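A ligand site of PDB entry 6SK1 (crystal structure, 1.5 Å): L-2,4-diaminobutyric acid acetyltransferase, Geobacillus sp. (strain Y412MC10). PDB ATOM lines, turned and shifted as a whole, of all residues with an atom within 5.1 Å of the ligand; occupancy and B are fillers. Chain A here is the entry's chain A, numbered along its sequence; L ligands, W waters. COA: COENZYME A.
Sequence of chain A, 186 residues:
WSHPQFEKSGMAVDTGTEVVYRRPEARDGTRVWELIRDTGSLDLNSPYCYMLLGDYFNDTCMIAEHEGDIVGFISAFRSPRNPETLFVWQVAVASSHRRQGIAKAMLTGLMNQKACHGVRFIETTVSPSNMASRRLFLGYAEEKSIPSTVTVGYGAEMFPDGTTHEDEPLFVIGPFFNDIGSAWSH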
ATOM      1  N   THR A  39      36.514  23.498   2.391  1.00  0.00           N
ATOM      2  CA  THR A  39      35.324  22.978   3.016  1.00  0.00           C
ATOM      3  C   THR A  39      35.047  23.724   4.343  1.00  0.00           C
ATOM      4  O   THR A  39      33.926  23.536   4.826  1.00  0.00           O
ATOM      5  CB  THR A  39      35.268  21.489   3.252  1.00  0.00           C
ATOM      6  OG1 THR A  39      36.219  21.200   4.339  1.00  0.00           O
ATOM      7  CG2 THR A  39      35.543  20.647   2.071  1.00  0.00           C
ATOM      8  N   TRP A  89      39.383   8.109   7.557  1.00  0.00           N
ATOM      9  CA  TRP A  89      39.484   9.235   8.483  1.00  0.00           C
ATOM     10  C   TRP A  89      39.155  10.572   7.904  1.00  0.00           C
ATOM     11  O   TRP A  89      38.967  11.499   8.675  1.00  0.00           O
ATOM     12  CB  TRP A  89      40.682   9.223   9.233  1.00  0.00           C
ATOM     13  CG  TRP A  89      41.930   9.400   8.474  1.00  0.00           C
ATOM     14  CD1 TRP A  89      42.569   8.480   7.711  1.00  0.00           C
ATOM     15  CD2 TRP A  89      42.880  10.486   8.718  1.00  0.00           C
ATOM     16  NE1 TRP A  89      43.782   9.007   7.245  1.00  0.00           N
ATOM     17  CE2 TRP A  89      44.049  10.223   7.893  1.00  0.00           C
ATOM     18  CE3 TRP A  89      42.896  11.674   9.597  1.00  0.00           C
ATOM     19  CZ2 TRP A  89      45.196  11.060   7.905  1.00  0.00           C
ATOM     20  CZ3 TRP A  89      44.012  12.469   9.544  1.00  0.00           C
ATOM     21  CH2 TRP A  89      45.196  12.171   8.734  1.00  0.00           C
ATOM     22  N   GLN A  90      39.148  10.708   6.579  1.00  0.00           N
ATOM     23  CA  GLN A  90      38.704  11.962   5.992  1.00  0.00           C
ATOM     24  C   GLN A  90      38.006  11.704   4.704  1.00  0.00           C
ATOM     25  O   GLN A  90      38.456  10.888   3.882  1.00  0.00           O
ATOM     26  CB  GLN A  90      39.870  12.910   5.756  1.00  0.00           C
ATOM     27  CG  GLN A  90      39.529  14.384   5.544  1.00  0.00           C
ATOM     28  CD  GLN A  90      40.654  15.365   6.224  1.00  0.00           C
ATOM     29  OE1 GLN A  90      41.940  15.163   6.174  1.00  0.00           O
ATOM     30  NE2 GLN A  90      40.148  16.388   6.977  1.00  0.00           N
ATOM     31  N   VAL A  91      36.872  12.390   4.412  1.00  0.00           N
ATOM     32  CA  VAL A  91      36.201  12.356   3.114  1.00  0.00           C
ATOM     33  C   VAL A  91      35.788  13.777   2.876  1.00  0.00           C
ATOM     34  O   VAL A  91      35.246  14.417   3.769  1.00  0.00           O
ATOM     35  CB  VAL A  91      34.943  11.450   3.032  1.00  0.00           C
ATOM     36  CG1 VAL A  91      34.645  11.268   1.575  1.00  0.00           C
ATOM     37  CG2 VAL A  91      35.134  10.146   3.728  1.00  0.00           C
ATOM     38  N   ALA A  92      36.001  14.304   1.693  1.00  0.00           N
ATOM     39  CA  ALA A  92      35.674  15.717   1.344  1.00  0.00           C
ATOM     40  C   ALA A  92      35.297  15.766  -0.105  1.00  0.00           C
ATOM     41  O   ALA A  92      36.002  15.243  -0.953  1.00  0.00           O
ATOM     42  CB  ALA A  92      36.790  16.611   1.690  1.00  0.00           C
ATOM     43  N   VAL A  93      34.188  16.488  -0.423  1.00  0.00           N
ATOM     44  CA  VAL A  93      33.855  16.832  -1.791  1.00  0.00           C
ATOM     45  C   VAL A  93      33.616  18.321  -1.854  1.00  0.00           C
ATOM     46  O   VAL A  93      32.946  18.872  -0.943  1.00  0.00           O
ATOM     47  CB  VAL A  93      32.654  16.021  -2.240  1.00  0.00           C
ATOM     48  CG1 VAL A  93      32.082  16.543  -3.583  1.00  0.00           C
ATOM     49  CG2 VAL A  93      33.023  14.533  -2.375  1.00  0.00           C
ATOM     50  N   HIS A  97      30.235  20.455  -6.069  1.00  0.00           N
ATOM     51  CA  HIS A  97      30.111  19.182  -6.630  1.00  0.00           C
ATOM     52  C   HIS A  97      29.460  18.132  -5.717  1.00  0.00           C
ATOM     53  O   HIS A  97      29.454  17.003  -6.024  1.00  0.00           O
ATOM     54  CB  HIS A  97      31.519  18.660  -7.031  1.00  0.00           C
ATOM     55  CG  HIS A  97      32.106  19.388  -8.198  1.00  0.00           C
ATOM     56  ND1 HIS A  97      32.057  18.919  -9.475  1.00  0.00           N
ATOM     57  CD2 HIS A  97      32.766  20.543  -8.248  1.00  0.00           C
ATOM     58  CE1 HIS A  97      32.649  19.767 -10.292  1.00  0.00           C
ATOM     59  NE2 HIS A  97      33.040  20.794  -9.572  1.00  0.00           N
ATOM     60  N   ARG A  98      28.862  18.567  -4.633  1.00  0.00           N
ATOM     61  CA  ARG A  98      28.178  17.691  -3.712  1.00  0.00           C
ATOM     62  C   ARG A  98      26.887  17.154  -4.172  1.00  0.00           C
ATOM     63  O   ARG A  98      26.238  17.766  -5.083  1.00  0.00           O
ATOM     64  CB  ARG A  98      28.046  18.302  -2.309  1.00  0.00           C
ATOM     65  CG  ARG A  98      29.356  18.493  -1.581  1.00  0.00           C
ATOM     66  CD  ARG A  98      29.166  19.104  -0.206  1.00  0.00           C
ATOM     67  NE  ARG A  98      30.457  19.497   0.305  1.00  0.00           N
ATOM     68  CZ  ARG A  98      30.695  20.350   1.239  1.00  0.00           C
ATOM     69  NH1 ARG A  98      29.661  20.724   1.996  1.00  0.00           N
ATOM     70  NH2 ARG A  98      31.916  20.707   1.513  1.00  0.00           N
ATOM     71  N   ARG A  99      26.469  16.054  -3.664  1.00  0.00           N
ATOM     72  CA  ARG A  99      25.212  15.456  -3.973  1.00  0.00           C
ATOM     73  C   ARG A  99      25.073  15.067  -5.391  1.00  0.00           C
ATOM     74  O   ARG A  99      23.999  15.174  -6.029  1.00  0.00           O
ATOM     75  CB  ARG A  99      24.034  16.289  -3.464  1.00  0.00           C
ATOM     76  CG  ARG A  99      24.190  16.729  -2.024  1.00  0.00           C
ATOM     77  CD  ARG A  99      22.956  17.436  -1.383  1.00  0.00           C
ATOM     78  NE  ARG A  99      21.944  16.530  -1.091  1.00  0.00           N
ATOM     79  CZ  ARG A  99      20.875  16.817  -0.322  1.00  0.00           C
ATOM     80  NH1 ARG A  99      20.818  18.084   0.135  1.00  0.00           N
ATOM     81  NH2 ARG A  99      20.013  15.918   0.020  1.00  0.00           N
ATOM     82  N   GLN A 100      26.150  14.569  -5.946  1.00  0.00           N
ATOM     83  CA  GLN A 100      26.279  14.055  -7.324  1.00  0.00           C
ATOM     84  C   GLN A 100      26.815  12.642  -7.277  1.00  0.00           C
ATOM     85  O   GLN A 100      27.075  12.040  -8.372  1.00  0.00           O
ATOM     86  CB  GLN A 100      27.181  14.952  -8.151  1.00  0.00           C
ATOM     87  CG  GLN A 100      26.712  16.386  -8.391  1.00  0.00           C
ATOM     88  CD  GLN A 100      27.734  17.079  -9.280  1.00  0.00           C
ATOM     89  OE1 GLN A 100      28.568  16.414  -9.884  1.00  0.00           O
ATOM     90  NE2 GLN A 100      27.816  18.367  -9.168  1.00  0.00           N
ATOM     91  N   GLY A 101      26.987  12.018  -6.112  1.00  0.00           N
ATOM     92  CA  GLY A 101      27.497  10.646  -6.028  1.00  0.00           C
ATOM     93  C   GLY A 101      29.013  10.549  -5.999  1.00  0.00           C
ATOM     94  O   GLY A 101      29.487   9.375  -6.058  1.00  0.00           O
ATOM     95  N   ILE A 102      29.747  11.627  -5.894  1.00  0.00           N
ATOM     96  CA  ILE A 102      31.192  11.562  -5.938  1.00  0.00           C
ATOM     97  C   ILE A 102      31.757  10.844  -4.731  1.00  0.00           C
ATOM     98  O   ILE A 102      32.622   9.928  -4.863  1.00  0.00           O
ATOM     99  CB  ILE A 102      31.846  12.914  -6.132  1.00  0.00           C
ATOM    100  CG1 ILE A 102      31.427  13.488  -7.500  1.00  0.00           C
ATOM    101  CG2 ILE A 102      33.382  12.864  -5.987  1.00  0.00           C
ATOM    102  CD1 ILE A 102      31.833  14.879  -7.791  1.00  0.00           C
ATOM    103  N   ALA A 103      31.322  11.185  -3.520  1.00  0.00           N
ATOM    104  CA  ALA A 103      31.844  10.443  -2.354  1.00  0.00           C
ATOM    105  C   ALA A 103      31.510   9.012  -2.423  1.00  0.00           C
ATOM    106  O   ALA A 103      32.316   8.125  -2.081  1.00  0.00           O
ATOM    107  CB  ALA A 103      31.371  11.123  -1.070  1.00  0.00           C
ATOM    108  N   LYS A 104      30.294   8.633  -2.813  1.00  0.00           N
ATOM    109  CA  LYS A 104      29.891   7.262  -2.944  1.00  0.00           C
ATOM    110  C   LYS A 104      30.824   6.557  -3.933  1.00  0.00           C
ATOM    111  O   LYS A 104      31.198   5.410  -3.632  1.00  0.00           O
ATOM    112  CB  LYS A 104      28.437   7.183  -3.426  1.00  0.00           C
ATOM    113  CG  LYS A 104      27.882   5.825  -3.523  1.00  0.00           C
ATOM    114  CD  LYS A 104      26.497   5.798  -4.228  1.00  0.00           C
ATOM    115  CE  LYS A 104      25.493   6.604  -3.467  1.00  0.00           C
ATOM    116  NZ  LYS A 104      24.148   6.130  -3.922  1.00  0.00           N
ATOM    117  N   ALA A 105      31.128   7.185  -5.044  1.00  0.00           N
ATOM    118  CA  ALA A 105      32.022   6.560  -6.028  1.00  0.00           C
ATOM    119  C   ALA A 105      33.421   6.439  -5.467  1.00  0.00           C
ATOM    120  O   ALA A 105      34.099   5.401  -5.773  1.00  0.00           O
ATOM    121  CB  ALA A 105      32.042   7.356  -7.277  1.00  0.00           C
ATOM    122  N   ASN A 130      26.121  15.522  10.805  1.00  0.00           N
ATOM    123  CA  ASN A 130      26.661  15.331   9.456  1.00  0.00           C
ATOM    124  C   ASN A 130      25.881  14.275   8.766  1.00  0.00           C
ATOM    125  O   ASN A 130      26.263  13.110   8.616  1.00  0.00           O
ATOM    126  CB  ASN A 130      28.094  14.944   9.553  1.00  0.00           C
ATOM    127  CG  ASN A 130      28.811  15.056   8.225  1.00  0.00           C
ATOM    128  OD1 ASN A 130      28.183  15.151   7.184  1.00  0.00           O
ATOM    129  ND2 ASN A 130      30.168  15.146   8.271  1.00  0.00           N
ATOM    130  N   MET A 131      24.689  14.628   8.328  1.00  0.00           N
ATOM    131  CA  MET A 131      23.789  13.696   7.635  1.00  0.00           C
ATOM    132  C   MET A 131      24.430  13.165   6.319  1.00  0.00           C
ATOM    133  O   MET A 131      24.274  11.997   5.993  1.00  0.00           O
ATOM    134  CB  MET A 131      22.442  14.403   7.339  1.00  0.00           C
ATOM    135  CG  MET A 131      21.536  13.561   6.481  1.00  0.00           C
ATOM    136  SD  MET A 131      20.832  12.150   7.368  1.00  0.00           S
ATOM    137  CE  MET A 131      22.275  11.143   7.601  1.00  0.00           C
ATOM    138  N   ALA A 132      25.066  14.049   5.640  1.00  0.00           N
ATOM    139  CA  ALA A 132      25.694  13.681   4.328  1.00  0.00           C
ATOM    140  C   ALA A 132      26.678  12.508   4.541  1.00  0.00           C
ATOM    141  O   ALA A 132      26.630  11.519   3.821  1.00  0.00           O
ATOM    142  CB  ALA A 132      26.381  14.839   3.791  1.00  0.00           C
ATOM    143  N   SER A 133      27.530  12.644   5.548  1.00  0.00           N
ATOM    144  CA  SER A 133      28.492  11.579   5.790  1.00  0.00           C
ATOM    145  C   SER A 133      27.843  10.342   6.321  1.00  0.00           C
ATOM    146  O   SER A 133      28.135   9.198   5.964  1.00  0.00           O
ATOM    147  CB  SER A 133      29.569  12.128   6.695  1.00  0.00           C
ATOM    148  OG  SER A 133      30.526  11.086   6.857  1.00  0.00           O
ATOM    149  N   ARG A 135      24.849   9.279   5.687  1.00  0.00           N
ATOM    150  CA  ARG A 135      24.237   8.585   4.563  1.00  0.00           C
ATOM    151  C   ARG A 135      25.233   7.990   3.589  1.00  0.00           C
ATOM    152  O   ARG A 135      24.966   6.938   3.030  1.00  0.00           O
ATOM    153  CB  ARG A 135      23.262   9.535   3.852  1.00  0.00           C
ATOM    154  CG  ARG A 135      21.992   9.847   4.660  1.00  0.00           C
ATOM    155  CD  ARG A 135      21.244   8.687   5.186  1.00  0.00           C
ATOM    156  NE  ARG A 135      20.999   7.776   4.053  1.00  0.00           N
ATOM    157  CZ  ARG A 135      20.901   6.448   4.139  1.00  0.00           C
ATOM    158  NH1 ARG A 135      20.907   5.853   5.309  1.00  0.00           N
ATOM    159  NH2 ARG A 135      20.818   5.707   3.035  1.00  0.00           N
ATOM    160  N   LEU A 136      26.359   8.619   3.425  1.00  0.00           N
ATOM    161  CA  LEU A 136      27.461   8.000   2.643  1.00  0.00           C
ATOM    162  C   LEU A 136      27.757   6.646   3.185  1.00  0.00           C
ATOM    163  O   LEU A 136      27.735   5.616   2.428  1.00  0.00           O
ATOM    164  CB  LEU A 136      28.706   8.885   2.697  1.00  0.00           C
ATOM    165  CG  LEU A 136      29.971   8.267   2.092  1.00  0.00           C
ATOM    166  CD1 LEU A 136      29.778   7.961   0.623  1.00  0.00           C
ATOM    167  CD2 LEU A 136      31.154   9.153   2.359  1.00  0.00           C
ATOM    168  N   GLY A 139      24.489   4.310   3.668  1.00  0.00           N
ATOM    169  CA  GLY A 139      23.981   3.928   2.370  1.00  0.00           C
ATOM    170  C   GLY A 139      24.859   2.913   1.730  1.00  0.00           C
ATOM    171  O   GLY A 139      24.377   1.922   1.124  1.00  0.00           O
ATOM    172  N   TYR A 140      26.170   2.985   1.919  1.00  0.00           N
ATOM    173  CA  TYR A 140      27.047   1.953   1.365  1.00  0.00           C
ATOM    174  C   TYR A 140      26.777   0.657   2.048  1.00  0.00           C
ATOM    175  O   TYR A 140      26.679  -0.414   1.408  1.00  0.00           O
ATOM    176  CB  TYR A 140      28.526   2.396   1.607  1.00  0.00           C
ATOM    177  CG  TYR A 140      29.547   1.435   1.034  1.00  0.00           C
ATOM    178  CD1 TYR A 140      29.745   1.385  -0.312  1.00  0.00           C
ATOM    179  CD2 TYR A 140      30.237   0.573   1.863  1.00  0.00           C
ATOM    180  CE1 TYR A 140      30.659   0.468  -0.867  1.00  0.00           C
ATOM    181  CE2 TYR A 140      31.133  -0.380   1.341  1.00  0.00           C
ATOM    182  CZ  TYR A 140      31.338  -0.393   0.001  1.00  0.00           C
ATOM    183  OH  TYR A 140      32.243  -1.328  -0.475  1.00  0.00           O
ATOM    184  N   GLU A 142      24.005  -0.309   3.436  1.00  0.00           N
ATOM    185  CA  GLU A 142      22.609  -0.783   3.031  1.00  0.00           C
ATOM    186  C   GLU A 142      22.689  -1.394   1.678  1.00  0.00           C
ATOM    187  O   GLU A 142      22.100  -2.453   1.500  1.00  0.00           O
ATOM    188  CB  GLU A 142      21.648   0.383   3.046  1.00  0.00           C
ATOM    189  CG  GLU A 142      21.267   0.984   4.399  1.00  0.00           C
ATOM    190  CD  GLU A 142      20.651   2.397   4.302  1.00  0.00           C
ATOM    191  OE1 GLU A 142      20.469   3.015   5.378  1.00  0.00           O
ATOM    192  OE2 GLU A 142      20.414   2.908   3.193  1.00  0.00           O
HETATM  193  N1A COA L   1      21.646  15.506   2.976  1.00  0.00           N
HETATM  194  C2A COA L   1      21.160  14.304   2.943  1.00  0.00           C
HETATM  195  N3A COA L   1      21.646  13.257   2.295  1.00  0.00           N
HETATM  196  C4A COA L   1      22.815  13.549   1.675  1.00  0.00           C
HETATM  197  C5A COA L   1      23.432  14.795   1.649  1.00  0.00           C
HETATM  198  C6A COA L   1      22.814  15.876   2.367  1.00  0.00           C
HETATM  199  N6A COA L   1      23.318  17.087   2.411  1.00  0.00           N
HETATM  200  N7A COA L   1      24.611  14.746   0.928  1.00  0.00           N
HETATM  201  C8A COA L   1      24.615  13.488   0.562  1.00  0.00           C
HETATM  202  N9A COA L   1      23.623  12.741   0.952  1.00  0.00           N
HETATM  203  C1B COA L   1      23.447  11.339   0.742  1.00  0.00           C
HETATM  204  C2B COA L   1      23.260  10.868  -0.666  1.00  0.00           C
HETATM  205  O2B COA L   1      21.816  10.930  -0.972  1.00  0.00           O
HETATM  206  C3B COA L   1      23.848   9.492  -0.741  1.00  0.00           C
HETATM  207  O3B COA L   1      22.937   8.557  -0.098  1.00  0.00           O
HETATM  208  P3B COA L   1      22.685   7.052  -0.661  1.00  0.00           P
HETATM  209  O7A COA L   1      23.990   6.364  -0.465  1.00  0.00           O
HETATM  210  O8A COA L   1      21.471   6.591   0.234  1.00  0.00           O
HETATM  211  O9A COA L   1      22.305   7.257  -2.088  1.00  0.00           O
HETATM  212  C4B COA L   1      25.026   9.648   0.213  1.00  0.00           C
HETATM  213  O4B COA L   1      24.696  10.695   1.101  1.00  0.00           O
HETATM  214  C5B COA L   1      26.313  10.015  -0.441  1.00  0.00           C
HETATM  215  O5B COA L   1      26.125  11.047  -1.418  1.00  0.00           O
HETATM  216  P1A COA L   1      27.243  11.630  -2.325  1.00  0.00           P
HETATM  217  O1A COA L   1      26.590  12.513  -3.345  1.00  0.00           O
HETATM  218  O2A COA L   1      28.130  10.512  -2.801  1.00  0.00           O
HETATM  219  O3A COA L   1      28.051  12.539  -1.320  1.00  0.00           O
HETATM  220  P2A COA L   1      28.945  13.798  -1.658  1.00  0.00           P
HETATM  221  O4A COA L   1      29.751  13.518  -2.897  1.00  0.00           O
HETATM  222  O5A COA L   1      28.103  15.050  -1.651  1.00  0.00           O
HETATM  223  O6A COA L   1      29.960  13.856  -0.415  1.00  0.00           O
HETATM  224  CBP COA L   1      30.512  14.418   1.833  1.00  0.00           C
HETATM  225  CCP COA L   1      29.548  13.677   0.956  1.00  0.00           C
HETATM  226  CDP COA L   1      30.193  13.977   3.241  1.00  0.00           C
HETATM  227  CEP COA L   1      31.920  13.953   1.500  1.00  0.00           C
HETATM  228  CAP COA L   1      30.396  15.934   1.666  1.00  0.00           C
HETATM  229  OAP COA L   1      29.064  16.345   2.152  1.00  0.00           O
HETATM  230  C9P COA L   1      31.430  16.707   2.376  1.00  0.00           C
HETATM  231  O9P COA L   1      32.518  16.890   1.827  1.00  0.00           O
HETATM  232  N8P COA L   1      31.149  17.144   3.557  1.00  0.00           N
HETATM  233  C7P COA L   1      32.096  18.083   4.259  1.00  0.00           C
HETATM  234  C6P COA L   1      33.265  17.267   4.733  1.00  0.00           C
HETATM  235  C5P COA L   1      32.822  16.171   5.670  1.00  0.00           C
HETATM  236  O5P COA L   1      32.049  16.437   6.516  1.00  0.00           O
HETATM  237  N4P COA L   1      33.335  14.903   5.551  1.00  0.00           N
HETATM  238  C3P COA L   1      33.091  13.817   6.322  1.00  0.00           C
HETATM  239  C2P COA L   1      33.938  13.960   7.584  1.00  0.00           C
HETATM  240  S1P COA L   1      35.784  13.664   7.262  1.00  0.00           S
HETATM  241  O   HOH W   1      33.620  18.667   8.323  1.00  0.00           O
HETATM  242  O   HOH W   2      24.014  11.884  -4.088  1.00  0.00           O
HETATM  243  O   HOH W   3      36.453  15.311   9.628  1.00  0.00           O
HETATM  244  O   HOH W   4      19.686  12.994  -0.697  1.00  0.00           O
HETATM  245  O   HOH W   5      36.140  16.917   5.214  1.00  0.00           O
HETATM  246  O   HOH W   6      32.589  20.785   6.221  1.00  0.00           O
HETATM  247  O   HOH W   7      25.751  18.254   1.325  1.00  0.00           O
HETATM  248  O   HOH W   8      28.895  14.381  -5.251  1.00  0.00           O
HETATM  249  O   HOH W   9      19.581  11.543   1.661  1.00  0.00           O
HETATM  250  O   HOH W  10      28.781  17.233   5.387  1.00  0.00           O
HETATM  251  O   HOH W  11      26.983  16.051   0.437  1.00  0.00           O
HETATM  252  O   HOH W  12      20.287   8.995   1.455  1.00  0.00           O
HETATM  253  O   HOH W  13      21.797  13.697  -2.196  1.00  0.00           O
HETATM  254  O   HOH W  14      26.605   5.901  -0.158  1.00  0.00           O
HETATM  255  O   HOH W  15      24.073   3.806  -2.046  1.00  0.00           O
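NH2 of Arg 135 lies within salt-bridge range of OE2 of Glu 142 (2.8 Å). O of Val 93 is in hydrogen-bond range of NE of Arg 98 (2.9 Å). The side-chain amide oxygen (OD1) of Asn 130 lies within hydrogen-bond range of the backbone NH (N) of Ser 133 (3.1 Å).
The backbone NH (N) of Gln 100 lies within hydrogen-bond range of an oxygen (O1A) of the ligand. The backbone NH (N) of Val 93 lies within hydrogen-bond range of an oxygen (O9P) of the ligand (2.8 Å). The backbone NH (N) of Ala 103 lies within hydrogen-bond range of an oxygen (O4A) of the ligand, at 2.9 Å. A sulfur (S1P) of the ligand lies close to the backbone NH of Val 91, 3.3 Å away. The backbone carbonyl oxygen (O) of Val 91 lies within hydrogen-bond range of a nitrogen (N4P) of the ligand. The guanidinium group (NH2) of Arg 99 lies within hydrogen-bond range of a nitrogen (N1A) of the ligand (3.4 Å). The side-chain amino group of Lys 104 is in salt-bridge range of an oxygen (O9A) of the ligand (2.8 Å). The side-chain amide nitrogen (ND2) of Asn 130 is in hydrogen-bond range of an oxygen (O5P) of the ligand (2.9 Å). N of Arg 99 is in hydrogen-bond range of O5A of the ligand. The backbone NH of Gly 101 is in hydrogen-bond range of an oxygen (O1A) of the ligand, 2.8 Å away. The guanidinium group (NH2) of Arg 135 is in salt-bridge range of an oxygen (O8A) of the ligand, 3.0 Å away. N of Lys 104 is in hydrogen-bond range of O2A of the ligand (2.9 Å).
Water W14 lies within hydrogen-bond range of an oxygen (O7A) of the ligand and the backbone carbonyl oxygen (O) of Leu 136. Water W5 lies within hydrogen-bond range of O of Val 91 (3.0 Å) and N4P of the ligand (3.5 Å). Water W4 bridges an oxygen (O2B) of the ligand (3.0 Å) and the guanidinium group of Arg 99 (3.0 Å). Water W10 bridges OD1 of Asn 130 (2.8 Å) and N8P of the ligand (3.0 Å). Water W15 lies within hydrogen-bond range of NZ of Lys 104 (3.0 Å) and O7A of the ligand (3.0 Å). Water W13 lies within hydrogen-bond range of an oxygen (O2B) of the ligand (3.0 Å) and the guanidinium group of Arg 99 (3.0 Å).
O of Ala 132 sits close to O4B of the ligand, at 3.4 Å. Gln 90 touches the ligand (CA to S1P, 3.6 Å). CA of Ala 92 touches O9P of the ligand, 3.4 Å away. CB of Arg 98 touches O5A of the ligand, at 3.3 Å. Ile 102 touches the ligand (N to O4A, 3.5 Å). Met 131 touches the ligand. Ser 133 touches the ligand (N to CDP, 3.8 Å). Leu 136 touches the ligand. Gly 139 touches the ligand. Hydrophobic or aromatic side chains within 4 Å of the ligand: Val 91, Val 93, Ile 102, Ala 103, Met 131 and Ala 132. 18 residues have an atom within 4 Å of the ligand: Gln 90, Val 91, Ala 92, Val 93, Arg 98, Arg 99, Gln 100, Gly 101, Ile 102, Ala 103, Lys 104, Asn 130, Met 131, Ala 132, Ser 133, Arg 135, Leu 136 and Gly 139. Along chain A the residues within 4 Å of the ligand span positions 90 to 139. The nearest printed residue that does not touch the ligand is Trp 89 (4.1 Å).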
